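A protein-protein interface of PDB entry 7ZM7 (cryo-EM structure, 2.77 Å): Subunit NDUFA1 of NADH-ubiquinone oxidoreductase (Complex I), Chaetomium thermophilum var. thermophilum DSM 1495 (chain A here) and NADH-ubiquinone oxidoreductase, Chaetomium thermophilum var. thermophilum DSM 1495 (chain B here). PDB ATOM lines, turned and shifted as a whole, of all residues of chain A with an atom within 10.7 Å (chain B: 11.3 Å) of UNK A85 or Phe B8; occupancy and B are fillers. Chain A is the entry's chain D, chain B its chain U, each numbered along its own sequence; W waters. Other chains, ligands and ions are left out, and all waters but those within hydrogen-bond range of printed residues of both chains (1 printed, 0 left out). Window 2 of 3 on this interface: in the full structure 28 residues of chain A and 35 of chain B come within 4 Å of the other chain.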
ATOM      1  N   LYS A  80      13.110 -17.774  23.235  1.00  0.00           N
ATOM      2  CA  LYS A  80      13.700 -17.188  24.460  1.00  0.00           C
ATOM      3  C   LYS A  80      12.867 -16.017  24.989  1.00  0.00           C
ATOM      4  O   LYS A  80      12.289 -15.280  24.188  1.00  0.00           O
ATOM      5  CB  LYS A  80      15.170 -16.870  24.191  1.00  0.00           C
ATOM      6  CG  LYS A  80      16.023 -18.087  23.873  1.00  0.00           C
ATOM      7  CD  LYS A  80      17.361 -17.735  23.277  1.00  0.00           C
ATOM      8  CE  LYS A  80      18.381 -18.840  23.444  1.00  0.00           C
ATOM      9  NZ  LYS A  80      19.743 -18.376  23.093  1.00  0.00           N
ATOM     10  N   VAL A  81      12.775 -15.857  26.276  1.00  0.00           N
ATOM     11  CA  VAL A  81      11.984 -14.754  26.890  1.00  0.00           C
ATOM     12  C   VAL A  81      12.907 -13.951  27.802  1.00  0.00           C
ATOM     13  O   VAL A  81      13.760 -14.563  28.471  1.00  0.00           O
ATOM     14  CB  VAL A  81      10.709 -15.244  27.608  1.00  0.00           C
ATOM     15  CG1 VAL A  81       9.992 -16.340  26.848  1.00  0.00           C
ATOM     16  CG2 VAL A  81      10.963 -15.681  29.040  1.00  0.00           C
ATOM     17  N   UNK A  82      12.785 -12.651  27.797  1.00  0.00           N
ATOM     18  CA  UNK A  82      13.611 -11.743  28.566  1.00  0.00           C
ATOM     19  C   UNK A  82      12.711 -10.742  29.260  1.00  0.00           C
ATOM     20  O   UNK A  82      11.578 -10.500  28.845  1.00  0.00           O
ATOM     21  CB  UNK A  82      14.628 -11.009  27.684  1.00  0.00           C
ATOM     22  N   UNK A  83      13.230 -10.150  30.323  1.00  0.00           N
ATOM     23  CA  UNK A  83      12.489  -9.119  31.021  1.00  0.00           C
ATOM     24  C   UNK A  83      12.819  -7.715  30.546  1.00  0.00           C
ATOM     25  O   UNK A  83      11.918  -6.877  30.500  1.00  0.00           O
ATOM     26  CB  UNK A  83      12.738  -9.212  32.529  1.00  0.00           C
ATOM     27  N   UNK A  84      14.072  -7.434  30.189  1.00  0.00           N
ATOM     28  CA  UNK A  84      14.479  -6.047  30.011  1.00  0.00           C
ATOM     29  C   UNK A  84      14.907  -5.683  28.595  1.00  0.00           C
ATOM     30  O   UNK A  84      14.251  -4.859  27.950  1.00  0.00           O
ATOM     31  CB  UNK A  84      15.611  -5.707  30.982  1.00  0.00           C
ATOM     32  N   UNK A  85      15.990  -6.266  28.090  1.00  0.00           N
ATOM     33  CA  UNK A  85      16.620  -5.648  26.933  1.00  0.00           C
ATOM     34  C   UNK A  85      15.956  -6.095  25.644  1.00  0.00           C
ATOM     35  O   UNK A  85      15.422  -7.197  25.541  1.00  0.00           O
ATOM     36  CB  UNK A  85      18.113  -5.943  26.877  1.00  0.00           C
ATOM     37  N   UNK A  86      15.997  -5.212  24.658  1.00  0.00           N
ATOM     38  CA  UNK A  86      15.224  -5.367  23.455  1.00  0.00           C
ATOM     39  C   UNK A  86      15.519  -4.241  22.476  1.00  0.00           C
ATOM     40  O   UNK A  86      14.655  -3.842  21.701  1.00  0.00           O
ATOM     41  CB  UNK A  86      13.764  -5.410  23.782  1.00  0.00           C
ATOM     42  N   ALA B   2      10.617 -12.023  17.825  1.00  0.00           N
ATOM     43  CA  ALA B   2      11.519 -11.042  17.182  1.00  0.00           C
ATOM     44  C   ALA B   2      12.852 -11.679  16.807  1.00  0.00           C
ATOM     45  O   ALA B   2      13.240 -12.648  17.457  1.00  0.00           O
ATOM     46  CB  ALA B   2      11.709  -9.877  18.116  1.00  0.00           C
ATOM     47  N   THR B   3      13.551 -11.106  15.826  1.00  0.00           N
ATOM     48  CA  THR B   3      14.822 -11.711  15.342  1.00  0.00           C
ATOM     49  C   THR B   3      16.014 -11.128  16.100  1.00  0.00           C
ATOM     50  O   THR B   3      17.148 -11.464  15.748  1.00  0.00           O
ATOM     51  CB  THR B   3      14.985 -11.519  13.831  1.00  0.00           C
ATOM     52  OG1 THR B   3      14.789 -10.135  13.544  1.00  0.00           O
ATOM     53  CG2 THR B   3      14.021 -12.350  13.017  1.00  0.00           C
ATOM     54  N   ARG B   4      15.764 -10.268  17.080  1.00  0.00           N
ATOM     55  CA  ARG B   4      16.836  -9.604  17.861  1.00  0.00           C
ATOM     56  C   ARG B   4      17.651 -10.625  18.646  1.00  0.00           C
ATOM     57  O   ARG B   4      17.050 -11.539  19.209  1.00  0.00           O
ATOM     58  CB  ARG B   4      16.185  -8.648  18.856  1.00  0.00           C
ATOM     59  CG  ARG B   4      17.169  -7.900  19.738  1.00  0.00           C
ATOM     60  CD  ARG B   4      16.411  -7.200  20.839  1.00  0.00           C
ATOM     61  NE  ARG B   4      15.321  -7.998  21.383  1.00  0.00           N
ATOM     62  CZ  ARG B   4      15.408  -8.774  22.456  1.00  0.00           C
ATOM     63  NH1 ARG B   4      14.351  -9.448  22.870  1.00  0.00           N
ATOM     64  NH2 ARG B   4      16.548  -8.869  23.115  1.00  0.00           N
ATOM     65  N   LYS B   5      18.976 -10.458  18.685  1.00  0.00           N
ATOM     66  CA  LYS B   5      19.829 -11.338  19.518  1.00  0.00           C
ATOM     67  C   LYS B   5      19.482 -11.084  20.997  1.00  0.00           C
ATOM     68  O   LYS B   5      19.338  -9.900  21.349  1.00  0.00           O
ATOM     69  CB  LYS B   5      21.297 -11.024  19.258  1.00  0.00           C
ATOM     70  CG  LYS B   5      21.762 -11.163  17.816  1.00  0.00           C
ATOM     71  CD  LYS B   5      23.263 -11.018  17.677  1.00  0.00           C
ATOM     72  CE  LYS B   5      23.806  -9.812  18.415  1.00  0.00           C
ATOM     73  NZ  LYS B   5      25.280  -9.710  18.299  1.00  0.00           N
ATOM     74  N   PRO B   6      19.296 -12.098  21.884  1.00  0.00           N
ATOM     75  CA  PRO B   6      18.919 -11.822  23.261  1.00  0.00           C
ATOM     76  C   PRO B   6      20.114 -11.609  24.202  1.00  0.00           C
ATOM     77  O   PRO B   6      21.124 -12.244  24.006  1.00  0.00           O
ATOM     78  CB  PRO B   6      18.076 -13.054  23.592  1.00  0.00           C
ATOM     79  CG  PRO B   6      18.699 -14.176  22.795  1.00  0.00           C
ATOM     80  CD  PRO B   6      19.330 -13.527  21.582  1.00  0.00           C
ATOM     81  N   ALA B   7      19.980 -10.765  25.217  1.00  0.00           N
ATOM     82  CA  ALA B   7      21.134 -10.437  26.084  1.00  0.00           C
ATOM     83  C   ALA B   7      20.891 -10.910  27.515  1.00  0.00           C
ATOM     84  O   ALA B   7      21.862 -11.286  28.179  1.00  0.00           O
ATOM     85  CB  ALA B   7      21.359  -8.941  26.050  1.00  0.00           C
ATOM     86  N   PHE B   8      19.648 -10.867  27.972  1.00  0.00           N
ATOM     87  CA  PHE B   8      19.342 -11.216  29.379  1.00  0.00           C
ATOM     88  C   PHE B   8      18.271 -12.308  29.420  1.00  0.00           C
ATOM     89  O   PHE B   8      17.449 -12.285  30.340  1.00  0.00           O
ATOM     90  CB  PHE B   8      18.943  -9.961  30.158  1.00  0.00           C
ATOM     91  CG  PHE B   8      19.941  -8.835  30.104  1.00  0.00           C
ATOM     92  CD1 PHE B   8      21.068  -8.847  30.904  1.00  0.00           C
ATOM     93  CD2 PHE B   8      19.748  -7.759  29.257  1.00  0.00           C
ATOM     94  CE1 PHE B   8      21.986  -7.811  30.853  1.00  0.00           C
ATOM     95  CE2 PHE B   8      20.669  -6.728  29.202  1.00  0.00           C
ATOM     96  CZ  PHE B   8      21.785  -6.755  30.000  1.00  0.00           C
ATOM     97  N   ASN B   9      18.250 -13.193  28.428  1.00  0.00           N
ATOM     98  CA  ASN B   9      17.287 -14.324  28.412  1.00  0.00           C
ATOM     99  C   ASN B   9      17.637 -15.336  29.506  1.00  0.00           C
ATOM    100  O   ASN B   9      18.801 -15.718  29.602  1.00  0.00           O
ATOM    101  CB  ASN B   9      17.231 -15.000  27.045  1.00  0.00           C
ATOM    102  CG  ASN B   9      18.591 -15.253  26.431  1.00  0.00           C
ATOM    103  OD1 ASN B   9      19.462 -14.387  26.436  1.00  0.00           O
ATOM    104  ND2 ASN B   9      18.784 -16.442  25.892  1.00  0.00           N
ATOM    105  N   GLN B  10      16.646 -15.753  30.293  1.00  0.00           N
ATOM    106  CA  GLN B  10      16.871 -16.746  31.374  1.00  0.00           C
ATOM    107  C   GLN B  10      15.841 -17.878  31.265  1.00  0.00           C
ATOM    108  O   GLN B  10      16.055 -18.908  31.914  1.00  0.00           O
ATOM    109  CB  GLN B  10      16.807 -16.060  32.739  1.00  0.00           C
ATOM    110  CG  GLN B  10      17.864 -14.984  32.937  1.00  0.00           C
ATOM    111  CD  GLN B  10      19.263 -15.543  32.990  1.00  0.00           C
ATOM    112  OE1 GLN B  10      19.518 -16.572  33.608  1.00  0.00           O
ATOM    113  NE2 GLN B  10      20.189 -14.858  32.345  1.00  0.00           N
ATOM    114  N   HIS B  11      14.786 -17.698  30.464  1.00  0.00           N
ATOM    115  CA  HIS B  11      13.695 -18.709  30.358  1.00  0.00           C
ATOM    116  C   HIS B  11      13.308 -19.015  28.902  1.00  0.00           C
ATOM    117  O   HIS B  11      13.618 -18.202  28.041  1.00  0.00           O
ATOM    118  CB  HIS B  11      12.449 -18.290  31.168  1.00  0.00           C
ATOM    119  CG  HIS B  11      12.651 -18.068  32.626  1.00  0.00           C
ATOM    120  ND1 HIS B  11      12.915 -19.098  33.500  1.00  0.00           N
ATOM    121  CD2 HIS B  11      12.569 -16.949  33.373  1.00  0.00           C
ATOM    122  CE1 HIS B  11      13.021 -18.620  34.720  1.00  0.00           C
ATOM    123  NE2 HIS B  11      12.812 -17.303  34.668  1.00  0.00           N
ATOM    124  N   VAL B  12      12.680 -20.166  28.644  1.00  0.00           N
ATOM    125  CA  VAL B  12      12.197 -20.565  27.327  1.00  0.00           C
ATOM    126  C   VAL B  12      10.692 -20.751  27.403  1.00  0.00           C
ATOM    127  O   VAL B  12      10.185 -21.303  28.382  1.00  0.00           O
ATOM    128  CB  VAL B  12      12.888 -21.847  26.833  1.00  0.00           C
ATOM    129  CG1 VAL B  12      12.113 -22.453  25.702  1.00  0.00           C
ATOM    130  CG2 VAL B  12      14.298 -21.531  26.373  1.00  0.00           C
HETATM  131  O   HOH W   1      14.144 -12.469  24.377  1.00  0.00           O
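The backbone carbonyl oxygen (O) of His B11 sits at hydrogen-bond distance from the backbone NH (N) of Val A81, 3.1 Å away. The guanidinium group (NH2) of Arg B4 sits at hydrogen-bond distance from O of UNK A85, 3.2 Å away.
CG of Pro B6 touches CD of Lys A80, 3.8 Å away. Lys A80 touches Asn B9 (CD to ND2, 3.2 Å). Lys A80 touches His B11. Val A81 touches Asn B9. Val A81 touches Gln B10 (O to N, 3.6 Å). Phe B8 touches UNK A85 (CD2 to CB, 3.4 Å). UNK A86 touches Arg B4 (CA to NE, 3.4 Å).
Of the printed residues of chain B, Lys A80 touches Pro B6 (3.8 Å), Asn B9 (3.2 Å) and His B11 (3.7 Å). Of the printed residues of chain B, Val A81 touches Asn B9, Gln B10 and His B11. No residue of chain B comes within 4 Å of UNK A82. No residue of chain B comes within 4 Å of UNK A83. No residue of chain B comes within 4 Å of UNK A84. Of the printed residues of chain B, UNK A85 touches Arg B4 (3.2 Å) and Phe B8 (3.4 Å). UNK A86 touches one residue of chain B. Printed residues of chain A within 4 Å of Pro B6: Lys A80. No residue of chain A comes within 4 Å of Ala B7. Phe B8 touches just one residue of chain A: UNK A85. Of the printed residues of chain A, Asn B9 touches Lys A80 (3.2 Å) and Val A81 (3.5 Å). Of the printed residues of chain A, Gln B10 touches Val A81. Printed residues of chain A within 4 Å of His B11: Lys A80 and Val A81. The nearest printed residue of chain A that does not touch Gln B10 is UNK A82 (5.3 Å).
Printed residues of chain A that touch a printed residue of chain B: Lys A80, Val A81, UNK A85 and UNK A86. Hydrophobic or aromatic side chains of chain A within 4 Å of the printed part of chain B: Val A81. Of the 11 printed residues of chain B, 6 touch a printed residue of chain A. Printed residues of chain B that touch a printed residue of chain A: Arg B4, Pro B6, Phe B8, Asn B9, Gln B10 and His B11. Hydrophobic or aromatic side chains of chain B that line the printed part of chain A: Pro B6, Phe B8 and His B11. Along chain B the printed residues that touch a printed residue of chain A span positions 4 to 11. Among the printed residues, 9 pairs touch across the chains. Among the printed residues, no Asp or Glu carboxylate lies within 4 Å of a Lys or Arg side-chain nitrogen of the other chain.
Water W1 lies within hydrogen-bond range of O of Lys A80 (3.4 Å) and NH1 of Arg B4 (3.4 Å).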
